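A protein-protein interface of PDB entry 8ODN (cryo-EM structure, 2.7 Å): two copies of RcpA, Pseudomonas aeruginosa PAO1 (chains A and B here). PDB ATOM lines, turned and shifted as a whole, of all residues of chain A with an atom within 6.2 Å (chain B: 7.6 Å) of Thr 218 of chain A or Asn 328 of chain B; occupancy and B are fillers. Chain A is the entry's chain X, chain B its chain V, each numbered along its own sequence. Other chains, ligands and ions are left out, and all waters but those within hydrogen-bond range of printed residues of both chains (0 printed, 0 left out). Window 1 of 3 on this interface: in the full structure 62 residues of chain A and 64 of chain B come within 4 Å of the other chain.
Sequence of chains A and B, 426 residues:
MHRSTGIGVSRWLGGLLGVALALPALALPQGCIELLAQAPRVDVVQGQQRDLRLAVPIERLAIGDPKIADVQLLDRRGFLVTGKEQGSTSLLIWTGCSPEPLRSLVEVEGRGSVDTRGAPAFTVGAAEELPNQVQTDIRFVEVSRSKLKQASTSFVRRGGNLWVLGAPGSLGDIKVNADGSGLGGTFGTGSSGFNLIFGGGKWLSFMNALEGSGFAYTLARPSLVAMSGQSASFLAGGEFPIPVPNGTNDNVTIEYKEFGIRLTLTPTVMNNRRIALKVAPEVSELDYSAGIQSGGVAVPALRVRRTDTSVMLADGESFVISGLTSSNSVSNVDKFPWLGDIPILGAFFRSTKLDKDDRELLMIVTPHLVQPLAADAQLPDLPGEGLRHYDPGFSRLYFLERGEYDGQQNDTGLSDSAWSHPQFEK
O of Leu 219 of chain A lies close to OG of Ser 326 of chain B (3.4 Å). O of Ser 327 of chain B sits at hydrogen-bond distance from N of Leu 219 of chain A (2.8 Å). N of Tyr 217 of chain A lies within hydrogen-bond range of O of Ser 329 of chain B (2.7 Å).
Among the printed residues, merely in contact across the chains: Ala 216 of chain A with Ser 329 of chain B (3.3 Å), Tyr 217 of chain A with Asn 328 of chain B (3.4 Å), Thr 218 of chain A with Ser 327 of chain B (3.5 Å) and Thr 218 of chain A with Asn 328 of chain B (3.5 Å).
Printed residues of chain B within 4 Å of Tyr 217 of chain A: Asn 328 (3.4 Å) and Ser 329 (2.7 Å). Of chain B, only Ser 327 and Asn 328 come within 4 Å of Thr 218 of chain A. Printed residues of chain B within 4 Å of Leu 219 of chain A: Ser 326 and Ser 327. Asn 328 of chain B touches two residues of chain A. Val 330 of chain B touches none of the printed residues of chain A. Lys 356 of chain B touches none of the printed residues of chain A. The nearest residue of chain A that does not touch Asn 328 of chain B is Leu 219 of chain A (4.6 Å). The nearest printed residue of chain A that does not touch Ser 327 of chain B is Tyr 217 of chain A (4.2 Å).
Of the 13 printed residues of chain B, 4 touch a printed residue of chain A.
No position is printed for both chains.
The side-chain hydroxyl (OG) of Ser 326 of chain B lies within hydrogen-bond range of the side-chain amide oxygen (OD1) of Asn 328 of chain B, 3.4 Å away. O of Arg 359 of chain B sits at hydrogen-bond distance from N of Ser 326 of chain B (3.2 Å). The side-chain carboxylate of Asp 358 of chain B sits at hydrogen-bond distance from the side-chain hydroxyl of Ser 327 of chain B (2.9 Å). The backbone NH (N) of Asp 357 of chain B sits at hydrogen-bond distance from the backbone carbonyl oxygen (O) of Asn 328 of chain B (2.9 Å). The backbone NH of Thr 218 of chain A is in hydrogen-bond range of the backbone carbonyl oxygen of Glu 142 of chain A, at 3.0 Å.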
ATOM      1  N   PHE A 140      -3.330 -28.699  -8.536  1.00  0.00           N
ATOM      2  CA  PHE A 140      -2.532 -27.561  -8.963  1.00  0.00           C
ATOM      3  C   PHE A 140      -3.105 -26.284  -8.372  1.00  0.00           C
ATOM      4  O   PHE A 140      -4.319 -26.068  -8.396  1.00  0.00           O
ATOM      5  CB  PHE A 140      -2.493 -27.461 -10.491  1.00  0.00           C
ATOM      6  CG  PHE A 140      -1.912 -26.175 -11.001  1.00  0.00           C
ATOM      7  CD1 PHE A 140      -2.728 -25.094 -11.279  1.00  0.00           C
ATOM      8  CD2 PHE A 140      -0.552 -26.049 -11.205  1.00  0.00           C
ATOM      9  CE1 PHE A 140      -2.198 -23.912 -11.746  1.00  0.00           C
ATOM     10  CE2 PHE A 140      -0.016 -24.870 -11.673  1.00  0.00           C
ATOM     11  CZ  PHE A 140      -0.840 -23.800 -11.943  1.00  0.00           C
ATOM     12  N   VAL A 141      -2.224 -25.437  -7.848  1.00  0.00           N
ATOM     13  CA  VAL A 141      -2.613 -24.162  -7.260  1.00  0.00           C
ATOM     14  C   VAL A 141      -1.600 -23.109  -7.677  1.00  0.00           C
ATOM     15  O   VAL A 141      -0.389 -23.354  -7.656  1.00  0.00           O
ATOM     16  CB  VAL A 141      -2.704 -24.240  -5.722  1.00  0.00           C
ATOM     17  CG1 VAL A 141      -3.293 -22.957  -5.160  1.00  0.00           C
ATOM     18  CG2 VAL A 141      -3.522 -25.440  -5.289  1.00  0.00           C
ATOM     19  N   GLU A 142      -2.095 -21.936  -8.058  1.00  0.00           N
ATOM     20  CA  GLU A 142      -1.239 -20.801  -8.371  1.00  0.00           C
ATOM     21  C   GLU A 142      -1.848 -19.543  -7.778  1.00  0.00           C
ATOM     22  O   GLU A 142      -3.042 -19.287  -7.953  1.00  0.00           O
ATOM     23  CB  GLU A 142      -1.057 -20.634  -9.881  1.00  0.00           C
ATOM     24  CG  GLU A 142      -0.185 -19.449 -10.264  1.00  0.00           C
ATOM     25  CD  GLU A 142      -0.036 -19.293 -11.760  1.00  0.00           C
ATOM     26  OE1 GLU A 142      -0.991 -19.631 -12.488  1.00  0.00           O
ATOM     27  OE2 GLU A 142       1.035 -18.835 -12.209  1.00  0.00           O
ATOM     28  N   VAL A 143      -1.025 -18.763  -7.088  1.00  0.00           N
ATOM     29  CA  VAL A 143      -1.422 -17.470  -6.550  1.00  0.00           C
ATOM     30  C   VAL A 143      -0.396 -16.439  -6.992  1.00  0.00           C
ATOM     31  O   VAL A 143       0.813 -16.667  -6.883  1.00  0.00           O
ATOM     32  CB  VAL A 143      -1.537 -17.502  -5.012  1.00  0.00           C
ATOM     33  CG1 VAL A 143      -2.062 -16.181  -4.488  1.00  0.00           C
ATOM     34  CG2 VAL A 143      -2.436 -18.640  -4.577  1.00  0.00           C
ATOM     35  N   ALA A 216      -4.716 -12.793  -8.570  1.00  0.00           N
ATOM     36  CA  ALA A 216      -5.142 -13.887  -9.426  1.00  0.00           C
ATOM     37  C   ALA A 216      -5.000 -15.197  -8.671  1.00  0.00           C
ATOM     38  O   ALA A 216      -4.040 -15.391  -7.920  1.00  0.00           O
ATOM     39  CB  ALA A 216      -4.327 -13.936 -10.720  1.00  0.00           C
ATOM     40  N   TYR A 217      -5.961 -16.094  -8.877  1.00  0.00           N
ATOM     41  CA  TYR A 217      -5.987 -17.386  -8.213  1.00  0.00           C
ATOM     42  C   TYR A 217      -6.450 -18.440  -9.205  1.00  0.00           C
ATOM     43  O   TYR A 217      -7.355 -18.192 -10.006  1.00  0.00           O
ATOM     44  CB  TYR A 217      -6.910 -17.356  -6.989  1.00  0.00           C
ATOM     45  CG  TYR A 217      -7.139 -18.701  -6.339  1.00  0.00           C
ATOM     46  CD1 TYR A 217      -8.184 -19.520  -6.743  1.00  0.00           C
ATOM     47  CD2 TYR A 217      -6.321 -19.147  -5.314  1.00  0.00           C
ATOM     48  CE1 TYR A 217      -8.400 -20.746  -6.151  1.00  0.00           C
ATOM     49  CE2 TYR A 217      -6.529 -20.372  -4.716  1.00  0.00           C
ATOM     50  CZ  TYR A 217      -7.570 -21.166  -5.137  1.00  0.00           C
ATOM     51  OH  TYR A 217      -7.779 -22.387  -4.539  1.00  0.00           O
ATOM     52  N   THR A 218      -5.826 -19.613  -9.148  1.00  0.00           N
ATOM     53  CA  THR A 218      -6.147 -20.709 -10.047  1.00  0.00           C
ATOM     54  C   THR A 218      -6.090 -22.020  -9.282  1.00  0.00           C
ATOM     55  O   THR A 218      -5.199 -22.227  -8.454  1.00  0.00           O
ATOM     56  CB  THR A 218      -5.184 -20.757 -11.240  1.00  0.00           C
ATOM     57  OG1 THR A 218      -5.320 -19.561 -12.019  1.00  0.00           O
ATOM     58  CG2 THR A 218      -5.471 -21.964 -12.116  1.00  0.00           C
ATOM     59  N   LEU A 219      -7.047 -22.901  -9.564  1.00  0.00           N
ATOM     60  CA  LEU A 219      -7.112 -24.214  -8.941  1.00  0.00           C
ATOM     61  C   LEU A 219      -7.621 -25.214  -9.964  1.00  0.00           C
ATOM     62  O   LEU A 219      -8.587 -24.935 -10.678  1.00  0.00           O
ATOM     63  CB  LEU A 219      -8.025 -24.196  -7.709  1.00  0.00           C
ATOM     64  CG  LEU A 219      -8.326 -25.540  -7.044  1.00  0.00           C
ATOM     65  CD1 LEU A 219      -7.064 -26.167  -6.495  1.00  0.00           C
ATOM     66  CD2 LEU A 219      -9.352 -25.364  -5.943  1.00  0.00           C
ATOM     67  N   ALA A 220      -6.969 -26.371 -10.035  1.00  0.00           N
ATOM     68  CA  ALA A 220      -7.359 -27.418 -10.966  1.00  0.00           C
ATOM     69  C   ALA A 220      -7.080 -28.768 -10.327  1.00  0.00           C
ATOM     70  O   ALA A 220      -5.991 -28.993  -9.795  1.00  0.00           O
ATOM     71  CB  ALA A 220      -6.607 -27.292 -12.293  1.00  0.00           C
ATOM     72  N   VAL A 283      -1.251 -26.584 -17.396  1.00  0.00           N
ATOM     73  CA  VAL A 283      -2.337 -25.635 -17.179  1.00  0.00           C
ATOM     74  C   VAL A 283      -2.001 -24.384 -17.974  1.00  0.00           C
ATOM     75  O   VAL A 283      -1.052 -23.668 -17.635  1.00  0.00           O
ATOM     76  CB  VAL A 283      -2.534 -25.290 -15.692  1.00  0.00           C
ATOM     77  CG1 VAL A 283      -3.640 -24.259 -15.530  1.00  0.00           C
ATOM     78  CG2 VAL A 283      -2.840 -26.538 -14.892  1.00  0.00           C
ATOM     79  N   GLU A 285      -3.554 -21.008 -20.699  1.00  0.00           N
ATOM     80  CA  GLU A 285      -4.663 -20.134 -21.047  1.00  0.00           C
ATOM     81  C   GLU A 285      -4.171 -19.101 -22.049  1.00  0.00           C
ATOM     82  O   GLU A 285      -2.967 -18.882 -22.201  1.00  0.00           O
ATOM     83  CB  GLU A 285      -5.253 -19.451 -19.809  1.00  0.00           C
ATOM     84  CG  GLU A 285      -4.245 -18.664 -18.998  1.00  0.00           C
ATOM     85  CD  GLU A 285      -4.850 -18.063 -17.747  1.00  0.00           C
ATOM     86  OE1 GLU A 285      -6.017 -17.623 -17.801  1.00  0.00           O
ATOM     87  OE2 GLU A 285      -4.160 -18.033 -16.707  1.00  0.00           O
ATOM     88  N   ARG A 303      -0.195 -18.337 -21.712  1.00  0.00           N
ATOM     89  CA  ARG A 303       0.366 -18.325 -20.367  1.00  0.00           C
ATOM     90  C   ARG A 303       0.378 -19.767 -19.873  1.00  0.00           C
ATOM     91  O   ARG A 303      -0.678 -20.339 -19.590  1.00  0.00           O
ATOM     92  CB  ARG A 303      -0.449 -17.415 -19.450  1.00  0.00           C
ATOM     93  CG  ARG A 303      -0.146 -17.562 -17.970  1.00  0.00           C
ATOM     94  CD  ARG A 303      -0.861 -16.495 -17.153  1.00  0.00           C
ATOM     95  NE  ARG A 303      -0.767 -16.748 -15.721  1.00  0.00           N
ATOM     96  CZ  ARG A 303      -1.139 -15.890 -14.781  1.00  0.00           C
ATOM     97  NH1 ARG A 303      -1.619 -14.695 -15.086  1.00  0.00           N
ATOM     98  NH2 ARG A 303      -1.023 -16.236 -13.503  1.00  0.00           N
ATOM     99  N   ARG A 305       1.922 -23.120 -17.617  1.00  0.00           N
ATOM    100  CA  ARG A 305       2.556 -23.695 -16.435  1.00  0.00           C
ATOM    101  C   ARG A 305       2.468 -25.208 -16.574  1.00  0.00           C
ATOM    102  O   ARG A 305       1.374 -25.774 -16.504  1.00  0.00           O
ATOM    103  CB  ARG A 305       1.876 -23.214 -15.151  1.00  0.00           C
ATOM    104  CG  ARG A 305       1.987 -21.718 -14.909  1.00  0.00           C
ATOM    105  CD  ARG A 305       0.647 -21.094 -14.558  1.00  0.00           C
ATOM    106  NE  ARG A 305      -0.314 -21.200 -15.650  1.00  0.00           N
ATOM    107  CZ  ARG A 305      -1.489 -20.585 -15.677  1.00  0.00           C
ATOM    108  NH1 ARG A 305      -1.881 -19.796 -14.691  1.00  0.00           N
ATOM    109  NH2 ARG A 305      -2.290 -20.765 -16.722  1.00  0.00           N
ATOM    110  N   ARG B 145     -19.857 -22.292 -14.316  1.00  0.00           N
ATOM    111  CA  ARG B 145     -20.448 -21.033 -13.895  1.00  0.00           C
ATOM    112  C   ARG B 145     -19.395 -19.940 -13.988  1.00  0.00           C
ATOM    113  O   ARG B 145     -18.194 -20.199 -13.893  1.00  0.00           O
ATOM    114  CB  ARG B 145     -20.999 -21.113 -12.467  1.00  0.00           C
ATOM    115  CG  ARG B 145     -22.376 -21.737 -12.362  1.00  0.00           C
ATOM    116  CD  ARG B 145     -22.780 -21.926 -10.909  1.00  0.00           C
ATOM    117  NE  ARG B 145     -22.277 -23.183 -10.363  1.00  0.00           N
ATOM    118  CZ  ARG B 145     -23.026 -24.233 -10.054  1.00  0.00           C
ATOM    119  NH1 ARG B 145     -24.344 -24.216 -10.189  1.00  0.00           N
ATOM    120  NH2 ARG B 145     -22.439 -25.332  -9.588  1.00  0.00           N
ATOM    121  N   LYS B 147     -18.810 -15.379 -13.314  1.00  0.00           N
ATOM    122  CA  LYS B 147     -19.283 -14.084 -12.855  1.00  0.00           C
ATOM    123  C   LYS B 147     -18.339 -13.011 -13.376  1.00  0.00           C
ATOM    124  O   LYS B 147     -17.172 -13.275 -13.679  1.00  0.00           O
ATOM    125  CB  LYS B 147     -19.382 -14.014 -11.326  1.00  0.00           C
ATOM    126  CG  LYS B 147     -20.378 -14.996 -10.730  1.00  0.00           C
ATOM    127  CD  LYS B 147     -20.770 -14.621  -9.308  1.00  0.00           C
ATOM    128  CE  LYS B 147     -21.659 -13.386  -9.278  1.00  0.00           C
ATOM    129  NZ  LYS B 147     -22.229 -13.135  -7.926  1.00  0.00           N
ATOM    130  N   SER B 326     -12.361 -27.287 -11.362  1.00  0.00           N
ATOM    131  CA  SER B 326     -11.500 -26.158 -11.674  1.00  0.00           C
ATOM    132  C   SER B 326     -12.112 -24.881 -11.124  1.00  0.00           C
ATOM    133  O   SER B 326     -13.329 -24.780 -10.949  1.00  0.00           O
ATOM    134  CB  SER B 326     -11.281 -26.013 -13.185  1.00  0.00           C
ATOM    135  OG  SER B 326     -10.447 -24.906 -13.474  1.00  0.00           O
ATOM    136  N   SER B 327     -11.251 -23.905 -10.855  1.00  0.00           N
ATOM    137  CA  SER B 327     -11.697 -22.607 -10.375  1.00  0.00           C
ATOM    138  C   SER B 327     -10.635 -21.573 -10.711  1.00  0.00           C
ATOM    139  O   SER B 327      -9.443 -21.813 -10.510  1.00  0.00           O
ATOM    140  CB  SER B 327     -11.962 -22.633  -8.865  1.00  0.00           C
ATOM    141  OG  SER B 327     -12.448 -21.383  -8.412  1.00  0.00           O
ATOM    142  N   ASN B 328     -11.078 -20.426 -11.219  1.00  0.00           N
ATOM    143  CA  ASN B 328     -10.184 -19.338 -11.583  1.00  0.00           C
ATOM    144  C   ASN B 328     -10.763 -18.031 -11.070  1.00  0.00           C
ATOM    145  O   ASN B 328     -11.977 -17.814 -11.131  1.00  0.00           O
ATOM    146  CB  ASN B 328      -9.984 -19.258 -13.101  1.00  0.00           C
ATOM    147  CG  ASN B 328      -9.216 -20.442 -13.652  1.00  0.00           C
ATOM    148  OD1 ASN B 328      -9.691 -21.577 -13.616  1.00  0.00           O
ATOM    149  ND2 ASN B 328      -8.026 -20.179 -14.176  1.00  0.00           N
ATOM    150  N   SER B 329      -9.890 -17.164 -10.566  1.00  0.00           N
ATOM    151  CA  SER B 329     -10.291 -15.853 -10.080  1.00  0.00           C
ATOM    152  C   SER B 329      -9.240 -14.837 -10.492  1.00  0.00           C
ATOM    153  O   SER B 329      -8.041 -15.088 -10.345  1.00  0.00           O
ATOM    154  CB  SER B 329     -10.464 -15.850  -8.559  1.00  0.00           C
ATOM    155  OG  SER B 329     -11.388 -16.842  -8.147  1.00  0.00           O
ATOM    156  N   VAL B 330      -9.693 -13.701 -11.012  1.00  0.00           N
ATOM    157  CA  VAL B 330      -8.814 -12.615 -11.421  1.00  0.00           C
ATOM    158  C   VAL B 330      -9.442 -11.303 -10.980  1.00  0.00           C
ATOM    159  O   VAL B 330     -10.641 -11.080 -11.177  1.00  0.00           O
ATOM    160  CB  VAL B 330      -8.572 -12.621 -12.944  1.00  0.00           C
ATOM    161  CG1 VAL B 330      -7.699 -11.444 -13.338  1.00  0.00           C
ATOM    162  CG2 VAL B 330      -7.945 -13.938 -13.374  1.00  0.00           C
ATOM    163  N   LEU B 354     -13.402  -7.785 -12.134  1.00  0.00           N
ATOM    164  CA  LEU B 354     -13.430  -9.077 -11.462  1.00  0.00           C
ATOM    165  C   LEU B 354     -13.929 -10.132 -12.435  1.00  0.00           C
ATOM    166  O   LEU B 354     -14.945  -9.932 -13.105  1.00  0.00           O
ATOM    167  CB  LEU B 354     -14.324  -9.036 -10.217  1.00  0.00           C
ATOM    168  CG  LEU B 354     -14.714 -10.375  -9.587  1.00  0.00           C
ATOM    169  CD1 LEU B 354     -13.492 -11.177  -9.184  1.00  0.00           C
ATOM    170  CD2 LEU B 354     -15.613 -10.141  -8.387  1.00  0.00           C
ATOM    171  N   ASP B 355     -13.212 -11.250 -12.505  1.00  0.00           N
ATOM    172  CA  ASP B 355     -13.598 -12.376 -13.343  1.00  0.00           C
ATOM    173  C   ASP B 355     -13.415 -13.656 -12.547  1.00  0.00           C
ATOM    174  O   ASP B 355     -12.325 -13.914 -12.026  1.00  0.00           O
ATOM    175  CB  ASP B 355     -12.763 -12.424 -14.628  1.00  0.00           C
ATOM    176  CG  ASP B 355     -13.182 -13.546 -15.558  1.00  0.00           C
ATOM    177  OD1 ASP B 355     -14.182 -14.233 -15.257  1.00  0.00           O
ATOM    178  OD2 ASP B 355     -12.510 -13.744 -16.593  1.00  0.00           O
ATOM    179  N   LYS B 356     -14.476 -14.453 -12.458  1.00  0.00           N
ATOM    180  CA  LYS B 356     -14.445 -15.718 -11.744  1.00  0.00           C
ATOM    181  C   LYS B 356     -15.075 -16.794 -12.614  1.00  0.00           C
ATOM    182  O   LYS B 356     -15.981 -16.523 -13.404  1.00  0.00           O
ATOM    183  CB  LYS B 356     -15.178 -15.626 -10.398  1.00  0.00           C
ATOM    184  CG  LYS B 356     -15.336 -16.961  -9.692  1.00  0.00           C
ATOM    185  CD  LYS B 356     -15.923 -16.803  -8.298  1.00  0.00           C
ATOM    186  CE  LYS B 356     -14.891 -16.290  -7.311  1.00  0.00           C
ATOM    187  NZ  LYS B 356     -15.402 -16.297  -5.914  1.00  0.00           N
ATOM    188  N   ASP B 357     -14.583 -18.020 -12.462  1.00  0.00           N
ATOM    189  CA  ASP B 357     -15.064 -19.139 -13.256  1.00  0.00           C
ATOM    190  C   ASP B 357     -14.933 -20.420 -12.448  1.00  0.00           C
ATOM    191  O   ASP B 357     -14.006 -20.576 -11.649  1.00  0.00           O
ATOM    192  CB  ASP B 357     -14.292 -19.265 -14.575  1.00  0.00           C
ATOM    193  CG  ASP B 357     -14.796 -20.405 -15.439  1.00  0.00           C
ATOM    194  OD1 ASP B 357     -15.832 -21.008 -15.090  1.00  0.00           O
ATOM    195  OD2 ASP B 357     -14.152 -20.701 -16.468  1.00  0.00           O
ATOM    196  N   ASP B 358     -15.867 -21.339 -12.676  1.00  0.00           N
ATOM    197  CA  ASP B 358     -15.858 -22.646 -12.038  1.00  0.00           C
ATOM    198  C   ASP B 358     -16.321 -23.681 -13.052  1.00  0.00           C
ATOM    199  O   ASP B 358     -17.004 -23.359 -14.027  1.00  0.00           O
ATOM    200  CB  ASP B 358     -16.755 -22.681 -10.795  1.00  0.00           C
ATOM    201  CG  ASP B 358     -16.375 -21.631  -9.771  1.00  0.00           C
ATOM    202  OD1 ASP B 358     -15.166 -21.466  -9.506  1.00  0.00           O
ATOM    203  OD2 ASP B 358     -17.285 -20.968  -9.232  1.00  0.00           O
ATOM    204  N   ARG B 359     -15.938 -24.933 -12.817  1.00  0.00           N
ATOM    205  CA  ARG B 359     -16.218 -25.984 -13.782  1.00  0.00           C
ATOM    206  C   ARG B 359     -16.152 -27.340 -13.097  1.00  0.00           C
ATOM    207  O   ARG B 359     -15.412 -27.527 -12.128  1.00  0.00           O
ATOM    208  CB  ARG B 359     -15.228 -25.925 -14.948  1.00  0.00           C
ATOM    209  CG  ARG B 359     -15.493 -26.916 -16.060  1.00  0.00           C
ATOM    210  CD  ARG B 359     -14.394 -26.850 -17.099  1.00  0.00           C
ATOM    211  NE  ARG B 359     -14.227 -25.504 -17.632  1.00  0.00           N
ATOM    212  CZ  ARG B 359     -13.129 -25.066 -18.232  1.00  0.00           C
ATOM    213  NH1 ARG B 359     -12.063 -25.837 -18.375  1.00  0.00           N
ATOM    214  NH2 ARG B 359     -13.096 -23.820 -18.695  1.00  0.00           N
